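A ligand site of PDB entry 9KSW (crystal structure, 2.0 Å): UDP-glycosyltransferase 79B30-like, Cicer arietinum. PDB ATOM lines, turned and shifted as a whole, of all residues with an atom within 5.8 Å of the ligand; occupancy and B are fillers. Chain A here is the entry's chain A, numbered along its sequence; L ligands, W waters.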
ATOM      1  N   MET A  17       3.513  -2.365 -24.860  1.00  0.00           N
ATOM      2  CA  MET A  17       4.462  -1.259 -24.869  1.00  0.00           C
ATOM      3  C   MET A  17       5.797  -1.695 -25.460  1.00  0.00           C
ATOM      4  O   MET A  17       6.450  -0.930 -26.172  1.00  0.00           O
ATOM      5  CB  MET A  17       4.638  -0.715 -23.458  1.00  0.00           C
ATOM      6  CG  MET A  17       3.480   0.151 -22.898  1.00  0.00           C
ATOM      7  SD  MET A  17       2.620   1.196 -24.108  1.00  0.00           S
ATOM      8  CE  MET A  17       3.658   2.662 -24.038  1.00  0.00           C
ATOM      9  N   GLY A  18       6.211  -2.927 -25.187  1.00  0.00           N
ATOM     10  CA  GLY A  18       7.462  -3.437 -25.734  1.00  0.00           C
ATOM     11  C   GLY A  18       7.498  -3.539 -27.247  1.00  0.00           C
ATOM     12  O   GLY A  18       8.589  -3.641 -27.822  1.00  0.00           O
ATOM     13  N   ILE A  21       6.629   0.901 -28.682  1.00  0.00           N
ATOM     14  CA  ILE A  21       7.759   1.829 -28.569  1.00  0.00           C
ATOM     15  C   ILE A  21       8.787   1.603 -29.679  1.00  0.00           C
ATOM     16  O   ILE A  21       9.075   2.559 -30.426  1.00  0.00           O
ATOM     17  CB  ILE A  21       8.386   1.742 -27.160  1.00  0.00           C
ATOM     18  CG1 ILE A  21       7.522   2.473 -26.138  1.00  0.00           C
ATOM     19  CG2 ILE A  21       9.857   2.238 -27.156  1.00  0.00           C
ATOM     20  CD1 ILE A  21       7.865   2.135 -24.699  1.00  0.00           C
ATOM     21  N   PRO A  22       9.343   0.388 -29.881  1.00  0.00           N
ATOM     22  CA  PRO A  22      10.299   0.239 -30.997  1.00  0.00           C
ATOM     23  C   PRO A  22       9.700   0.446 -32.372  1.00  0.00           C
ATOM     24  O   PRO A  22      10.369   1.022 -33.229  1.00  0.00           O
ATOM     25  CB  PRO A  22      10.865  -1.182 -30.823  1.00  0.00           C
ATOM     26  CG  PRO A  22      10.018  -1.867 -29.858  1.00  0.00           C
ATOM     27  CD  PRO A  22       9.281  -0.821 -29.030  1.00  0.00           C
ATOM     28  N   ILE A 137      10.543  -7.385 -33.149  1.00  0.00           N
ATOM     29  CA  ILE A 137      11.488  -6.603 -32.352  1.00  0.00           C
ATOM     30  C   ILE A 137      12.150  -7.448 -31.267  1.00  0.00           C
ATOM     31  O   ILE A 137      12.836  -6.903 -30.398  1.00  0.00           O
ATOM     32  CB  ILE A 137      10.814  -5.342 -31.784  1.00  0.00           C
ATOM     33  CG1 ILE A 137       9.469  -5.680 -31.106  1.00  0.00           C
ATOM     34  CG2 ILE A 137      10.554  -4.324 -32.917  1.00  0.00           C
ATOM     35  CD1 ILE A 137       9.606  -6.334 -29.704  1.00  0.00           C
ATOM     36  N   TYR A 269      20.332   0.568 -10.809  1.00  0.00           N
ATOM     37  CA  TYR A 269      18.967   0.635 -11.329  1.00  0.00           C
ATOM     38  C   TYR A 269      18.484  -0.771 -11.677  1.00  0.00           C
ATOM     39  O   TYR A 269      19.131  -1.480 -12.459  1.00  0.00           O
ATOM     40  CB  TYR A 269      18.908   1.519 -12.576  1.00  0.00           C
ATOM     41  CG  TYR A 269      17.563   1.535 -13.273  1.00  0.00           C
ATOM     42  CD1 TYR A 269      16.477   2.221 -12.722  1.00  0.00           C
ATOM     43  CD2 TYR A 269      17.368   0.870 -14.475  1.00  0.00           C
ATOM     44  CE1 TYR A 269      15.228   2.230 -13.368  1.00  0.00           C
ATOM     45  CE2 TYR A 269      16.140   0.871 -15.113  1.00  0.00           C
ATOM     46  CZ  TYR A 269      15.065   1.563 -14.569  1.00  0.00           C
ATOM     47  OH  TYR A 269      13.827   1.575 -15.208  1.00  0.00           O
ATOM     48  N   GLY A 273      10.609  -4.828 -16.474  1.00  0.00           N
ATOM     49  CA  GLY A 273       9.564  -4.577 -17.456  1.00  0.00           C
ATOM     50  C   GLY A 273       8.230  -4.200 -16.821  1.00  0.00           C
ATOM     51  O   GLY A 273       8.141  -3.813 -15.656  1.00  0.00           O
ATOM     52  N   SER A 274       7.171  -4.328 -17.619  1.00  0.00           N
ATOM     53  CA  SER A 274       5.814  -3.992 -17.173  1.00  0.00           C
ATOM     54  C   SER A 274       4.839  -5.155 -17.391  1.00  0.00           C
ATOM     55  O   SER A 274       3.622  -4.943 -17.421  1.00  0.00           O
ATOM     56  CB  SER A 274       5.311  -2.762 -17.920  1.00  0.00           C
ATOM     57  OG  SER A 274       5.222  -3.064 -19.305  1.00  0.00           O
ATOM     58  N   ILE A 300      12.337  -0.660  -9.840  1.00  0.00           N
ATOM     59  CA  ILE A 300      11.021  -0.433 -10.436  1.00  0.00           C
ATOM     60  C   ILE A 300      10.361  -1.797 -10.599  1.00  0.00           C
ATOM     61  O   ILE A 300      10.693  -2.563 -11.516  1.00  0.00           O
ATOM     62  CB  ILE A 300      11.119   0.324 -11.762  1.00  0.00           C
ATOM     63  CG1 ILE A 300      11.917   1.622 -11.584  1.00  0.00           C
ATOM     64  CG2 ILE A 300       9.726   0.604 -12.321  1.00  0.00           C
ATOM     65  CD1 ILE A 300      11.372   2.475 -10.454  1.00  0.00           C
ATOM     66  N   GLY A 331       5.191   2.580 -10.222  1.00  0.00           N
ATOM     67  CA  GLY A 331       4.662   3.199 -11.420  1.00  0.00           C
ATOM     68  C   GLY A 331       5.563   3.027 -12.655  1.00  0.00           C
ATOM     69  O   GLY A 331       6.732   2.644 -12.577  1.00  0.00           O
ATOM     70  N   TRP A 332       4.959   3.311 -13.812  1.00  0.00           N
ATOM     71  CA  TRP A 332       5.696   3.462 -15.074  1.00  0.00           C
ATOM     72  C   TRP A 332       6.622   4.670 -14.993  1.00  0.00           C
ATOM     73  O   TRP A 332       6.185   5.768 -14.660  1.00  0.00           O
ATOM     74  CB  TRP A 332       4.704   3.655 -16.219  1.00  0.00           C
ATOM     75  CG  TRP A 332       5.321   3.831 -17.598  1.00  0.00           C
ATOM     76  CD1 TRP A 332       5.696   5.016 -18.192  1.00  0.00           C
ATOM     77  CD2 TRP A 332       5.601   2.804 -18.555  1.00  0.00           C
ATOM     78  NE1 TRP A 332       6.212   4.770 -19.456  1.00  0.00           N
ATOM     79  CE2 TRP A 332       6.150   3.423 -19.703  1.00  0.00           C
ATOM     80  CE3 TRP A 332       5.439   1.412 -18.552  1.00  0.00           C
ATOM     81  CZ2 TRP A 332       6.541   2.692 -20.820  1.00  0.00           C
ATOM     82  CZ3 TRP A 332       5.831   0.700 -19.677  1.00  0.00           C
ATOM     83  CH2 TRP A 332       6.382   1.334 -20.786  1.00  0.00           C
ATOM     84  N   ILE A 333       7.909   4.484 -15.318  1.00  0.00           N
ATOM     85  CA  ILE A 333       8.836   5.610 -15.305  1.00  0.00           C
ATOM     86  C   ILE A 333       9.521   5.772 -16.656  1.00  0.00           C
ATOM     87  O   ILE A 333       9.294   4.975 -17.574  1.00  0.00           O
ATOM     88  CB  ILE A 333       9.852   5.476 -14.146  1.00  0.00           C
ATOM     89  CG1 ILE A 333      10.402   4.044 -14.029  1.00  0.00           C
ATOM     90  CG2 ILE A 333       9.225   5.897 -12.814  1.00  0.00           C
ATOM     91  CD1 ILE A 333      11.376   3.680 -15.059  1.00  0.00           C
ATOM     92  N   GLN A 334      10.332   6.811 -16.797  1.00  0.00           N
ATOM     93  CA  GLN A 334      11.021   7.116 -18.058  1.00  0.00           C
ATOM     94  C   GLN A 334      12.363   6.384 -18.069  1.00  0.00           C
ATOM     95  O   GLN A 334      13.421   6.974 -17.815  1.00  0.00           O
ATOM     96  CB  GLN A 334      11.190   8.623 -18.231  1.00  0.00           C
ATOM     97  CG  GLN A 334       9.885   9.389 -18.345  1.00  0.00           C
ATOM     98  CD  GLN A 334      10.088  10.883 -18.087  1.00  0.00           C
ATOM     99  OE1 GLN A 334      10.293  11.310 -16.942  1.00  0.00           O
ATOM    100  NE2 GLN A 334      10.069  11.666 -19.151  1.00  0.00           N
ATOM    101  N   GLN A 335      12.308   5.075 -18.355  1.00  0.00           N
ATOM    102  CA  GLN A 335      13.488   4.234 -18.150  1.00  0.00           C
ATOM    103  C   GLN A 335      14.653   4.678 -19.024  1.00  0.00           C
ATOM    104  O   GLN A 335      15.808   4.698 -18.560  1.00  0.00           O
ATOM    105  CB  GLN A 335      13.164   2.764 -18.446  1.00  0.00           C
ATOM    106  CG  GLN A 335      14.388   1.884 -18.575  1.00  0.00           C
ATOM    107  CD  GLN A 335      14.035   0.407 -18.490  1.00  0.00           C
ATOM    108  OE1 GLN A 335      13.509  -0.042 -17.481  1.00  0.00           O
ATOM    109  NE2 GLN A 335      14.296  -0.344 -19.569  1.00  0.00           N
ATOM    110  N   GLN A 336      14.380   5.023 -20.275  1.00  0.00           N
ATOM    111  CA  GLN A 336      15.465   5.435 -21.156  1.00  0.00           C
ATOM    112  C   GLN A 336      16.150   6.682 -20.611  1.00  0.00           C
ATOM    113  O   GLN A 336      17.377   6.793 -20.662  1.00  0.00           O
ATOM    114  CB  GLN A 336      14.951   5.653 -22.573  1.00  0.00           C
ATOM    115  CG  GLN A 336      16.022   6.155 -23.528  1.00  0.00           C
ATOM    116  CD  GLN A 336      15.465   6.840 -24.753  1.00  0.00           C
ATOM    117  OE1 GLN A 336      14.464   6.399 -25.328  1.00  0.00           O
ATOM    118  NE2 GLN A 336      16.102   7.924 -25.157  1.00  0.00           N
ATOM    119  N   HIS A 350      15.636  -7.572 -16.648  1.00  0.00           N
ATOM    120  CA  HIS A 350      14.980  -8.834 -16.985  1.00  0.00           C
ATOM    121  C   HIS A 350      15.346  -9.350 -18.377  1.00  0.00           C
ATOM    122  O   HIS A 350      14.905 -10.447 -18.756  1.00  0.00           O
ATOM    123  CB  HIS A 350      13.464  -8.673 -16.890  1.00  0.00           C
ATOM    124  CG  HIS A 350      12.878  -7.849 -17.990  1.00  0.00           C
ATOM    125  ND1 HIS A 350      13.325  -6.576 -18.273  1.00  0.00           N
ATOM    126  CD2 HIS A 350      11.890  -8.112 -18.872  1.00  0.00           C
ATOM    127  CE1 HIS A 350      12.640  -6.095 -19.301  1.00  0.00           C
ATOM    128  NE2 HIS A 350      11.769  -7.005 -19.682  1.00  0.00           N
ATOM    129  N   CYS A 351      16.151  -8.594 -19.144  1.00  0.00           N
ATOM    130  CA  CYS A 351      16.660  -8.991 -20.460  1.00  0.00           C
ATOM    131  C   CYS A 351      15.596  -8.974 -21.570  1.00  0.00           C
ATOM    132  O   CYS A 351      15.748  -9.678 -22.577  1.00  0.00           O
ATOM    133  CB  CYS A 351      17.339 -10.369 -20.405  1.00  0.00           C
ATOM    134  SG  CYS A 351      18.734 -10.426 -19.239  1.00  0.00           S
ATOM    135  N   GLY A 352      14.531  -8.197 -21.407  1.00  0.00           N
ATOM    136  CA  GLY A 352      13.664  -7.890 -22.545  1.00  0.00           C
ATOM    137  C   GLY A 352      14.430  -7.208 -23.663  1.00  0.00           C
ATOM    138  O   GLY A 352      15.449  -6.545 -23.446  1.00  0.00           O
ATOM    139  N   ALA A 353      13.939  -7.394 -24.898  1.00  0.00           N
ATOM    140  CA  ALA A 353      14.676  -6.936 -26.067  1.00  0.00           C
ATOM    141  C   ALA A 353      14.883  -5.421 -26.053  1.00  0.00           C
ATOM    142  O   ALA A 353      15.934  -4.935 -26.460  1.00  0.00           O
ATOM    143  CB  ALA A 353      13.947  -7.363 -27.347  1.00  0.00           C
ATOM    144  N   GLY A 354      13.878  -4.661 -25.601  1.00  0.00           N
ATOM    145  CA  GLY A 354      14.035  -3.206 -25.582  1.00  0.00           C
ATOM    146  C   GLY A 354      14.991  -2.752 -24.496  1.00  0.00           C
ATOM    147  O   GLY A 354      15.836  -1.881 -24.728  1.00  0.00           O
ATOM    148  N   SER A 355      14.875  -3.346 -23.305  1.00  0.00           N
ATOM    149  CA  SER A 355      15.775  -3.001 -22.203  1.00  0.00           C
ATOM    150  C   SER A 355      17.211  -3.359 -22.532  1.00  0.00           C
ATOM    151  O   SER A 355      18.146  -2.652 -22.139  1.00  0.00           O
ATOM    152  CB  SER A 355      15.326  -3.693 -20.903  1.00  0.00           C
ATOM    153  OG  SER A 355      14.011  -3.286 -20.542  1.00  0.00           O
ATOM    154  N   ILE A 356      17.418  -4.465 -23.269  1.00  0.00           N
ATOM    155  CA  ILE A 356      18.768  -4.848 -23.673  1.00  0.00           C
ATOM    156  C   ILE A 356      19.406  -3.740 -24.500  1.00  0.00           C
ATOM    157  O   ILE A 356      20.529  -3.314 -24.214  1.00  0.00           O
ATOM    158  CB  ILE A 356      18.749  -6.170 -24.467  1.00  0.00           C
ATOM    159  CG1 ILE A 356      18.480  -7.386 -23.560  1.00  0.00           C
ATOM    160  CG2 ILE A 356      20.107  -6.375 -25.154  1.00  0.00           C
ATOM    161  CD1 ILE A 356      19.513  -7.570 -22.465  1.00  0.00           C
ATOM    162  N   GLU A 358      18.560  -0.577 -24.705  1.00  0.00           N
ATOM    163  CA  GLU A 358      18.718   0.638 -23.913  1.00  0.00           C
ATOM    164  C   GLU A 358      19.931   0.557 -22.994  1.00  0.00           C
ATOM    165  O   GLU A 358      20.592   1.570 -22.764  1.00  0.00           O
ATOM    166  CB  GLU A 358      17.429   0.915 -23.120  1.00  0.00           C
ATOM    167  CG  GLU A 358      16.352   1.559 -23.985  1.00  0.00           C
ATOM    168  CD  GLU A 358      14.918   1.282 -23.492  1.00  0.00           C
ATOM    169  OE1 GLU A 358      14.739   0.980 -22.281  1.00  0.00           O
ATOM    170  OE2 GLU A 358      13.983   1.393 -24.321  1.00  0.00           O
ATOM    171  N   TYR A 376      13.675 -13.537 -23.302  1.00  0.00           N
ATOM    172  CA  TYR A 376      14.497 -13.051 -22.186  1.00  0.00           C
ATOM    173  C   TYR A 376      15.668 -13.997 -21.949  1.00  0.00           C
ATOM    174  O   TYR A 376      16.818 -13.563 -21.854  1.00  0.00           O
ATOM    175  CB  TYR A 376      13.678 -12.925 -20.891  1.00  0.00           C
ATOM    176  CG  TYR A 376      12.439 -12.049 -20.856  1.00  0.00           C
ATOM    177  CD1 TYR A 376      12.052 -11.244 -21.946  1.00  0.00           C
ATOM    178  CD2 TYR A 376      11.652 -12.006 -19.708  1.00  0.00           C
ATOM    179  CE1 TYR A 376      10.910 -10.421 -21.866  1.00  0.00           C
ATOM    180  CE2 TYR A 376      10.529 -11.204 -19.625  1.00  0.00           C
ATOM    181  CZ  TYR A 376      10.165 -10.414 -20.695  1.00  0.00           C
ATOM    182  OH  TYR A 376       9.045  -9.642 -20.579  1.00  0.00           O
HETATM  183  N1  LIG L   1       9.612   0.833 -19.887  1.00  0.00           N
HETATM  184  C1  LIG L   1       9.504   2.153 -19.464  1.00  0.00           C
HETATM  185  N2  LIG L   1       9.132   2.302 -18.153  1.00  0.00           N
HETATM  186  C2  LIG L   1       8.799   1.298 -17.262  1.00  0.00           C
HETATM  187  C3  LIG L   1       8.902  -0.028 -17.781  1.00  0.00           C
HETATM  188  C4  LIG L   1       9.290  -0.215 -19.049  1.00  0.00           C
HETATM  189  O1  LIG L   1       9.769   3.102 -20.179  1.00  0.00           O
HETATM  190  O2  LIG L   1       8.464   1.616 -16.116  1.00  0.00           O
HETATM  191  C5  LIG L   1       9.990   0.621 -21.299  1.00  0.00           C
HETATM  192  C6  LIG L   1      11.422   0.134 -21.521  1.00  0.00           C
HETATM  193  O3  LIG L   1      12.323   1.220 -21.585  1.00  0.00           O
HETATM  194  C7  LIG L   1      11.275  -0.566 -22.882  1.00  0.00           C
HETATM  195  C8  LIG L   1       9.875  -1.202 -22.765  1.00  0.00           C
HETATM  196  O4  LIG L   1      11.310   0.372 -23.955  1.00  0.00           O
HETATM  197  O5  LIG L   1       9.139  -0.383 -21.829  1.00  0.00           O
HETATM  198  C9  LIG L   1       9.867  -2.619 -22.265  1.00  0.00           C
HETATM  199  O6  LIG L   1      10.370  -3.437 -23.339  1.00  0.00           O
HETATM  200  P1  LIG L   1      11.123  -4.802 -23.000  1.00  0.00           P
HETATM  201  O7  LIG L   1      10.178  -5.657 -22.150  1.00  0.00           O
HETATM  202  O8  LIG L   1      12.385  -4.438 -22.255  1.00  0.00           O
HETATM  203  O9  LIG L   1      11.376  -5.375 -24.390  1.00  0.00           O
HETATM  204  O   HOH W   1       8.546  -7.873 -22.349  1.00  0.00           O
HETATM  205  O   HOH W   2       9.515  -6.917 -25.712  1.00  0.00           O
HETATM  206  O   HOH W   3       7.852  -4.669 -20.385  1.00  0.00           O
HETATM  207  O   HOH W   4      11.051  -3.821 -26.858  1.00  0.00           O
HETATM  208  O   HOH W   5      11.638  -0.959 -26.497  1.00  0.00           O
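An oxygen (O3) of the ligand lies within hydrogen-bond range of the side-chain carboxylate (OE1) of Glu 358.
An oxygen (O8) of the ligand is in hydrogen-bond range of the backbone NH of Ser 355, at 2.9 Å.
The side-chain hydroxyl (OG) of Ser 355 is in hydrogen-bond range of an oxygen (O8) of the ligand (2.6 Å).
The backbone NH (N) of Ile 333 is in hydrogen-bond range of an oxygen (O2) of the ligand, at 3.0 Å.
The backbone carbonyl oxygen (O) of Ile 333 lies within hydrogen-bond range of a nitrogen (N2) of the ligand (2.7 Å).
The backbone NH (N) of Gly 354 sits at hydrogen-bond distance from an oxygen (O9) of the ligand.
An oxygen (O3) of the ligand is in hydrogen-bond range of the side-chain amide nitrogen of Gln 335.
NE2 of His 350 sits at hydrogen-bond distance from O7 of the ligand, 3.2 Å away.
N of Ala 353 lies within hydrogen-bond range of O9 of the ligand (3.3 Å).
The side-chain carboxylate of Glu 358 is in hydrogen-bond range of the side-chain amide nitrogen of Gln 335, 3.1 Å away.
The side-chain hydroxyl (OG) of Ser 355 lies within hydrogen-bond range of the side-chain amide nitrogen (NE2) of Gln 335 (3.1 Å).
The side-chain amide oxygen of Gln 335 sits at hydrogen-bond distance from the side-chain hydroxyl of Tyr 269, at 2.8 Å.
NE2 of His 350 lies close to N of Gly 352 (3.5 Å).
Merely in contact with the ligand: Gly 18 (3.8 Å), Ile 21 (3.9 Å), Trp 332 (3.3 Å) and Gly 352 (3.6 Å).
11 residues have an atom within 4 Å of the ligand: Gly 18, Ile 21, Trp 332, Ile 333, Gln 335, His 350, Gly 352, Ala 353, Gly 354, Ser 355 and Glu 358.
Water W1 lies within hydrogen-bond range of the side-chain hydroxyl (OH) of Tyr 376 (2.6 Å) and an oxygen (O7) of the ligand (2.8 Å).
Water W4 lies within hydrogen-bond range of O of Gly 18 (2.7 Å), O9 of the ligand (2.9 Å) and N of Gly 354 (3.2 Å).
Water W3 bridges the backbone NH (N) of Ser 274 (2.9 Å) and an oxygen (O7) of the ligand (3.1 Å).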
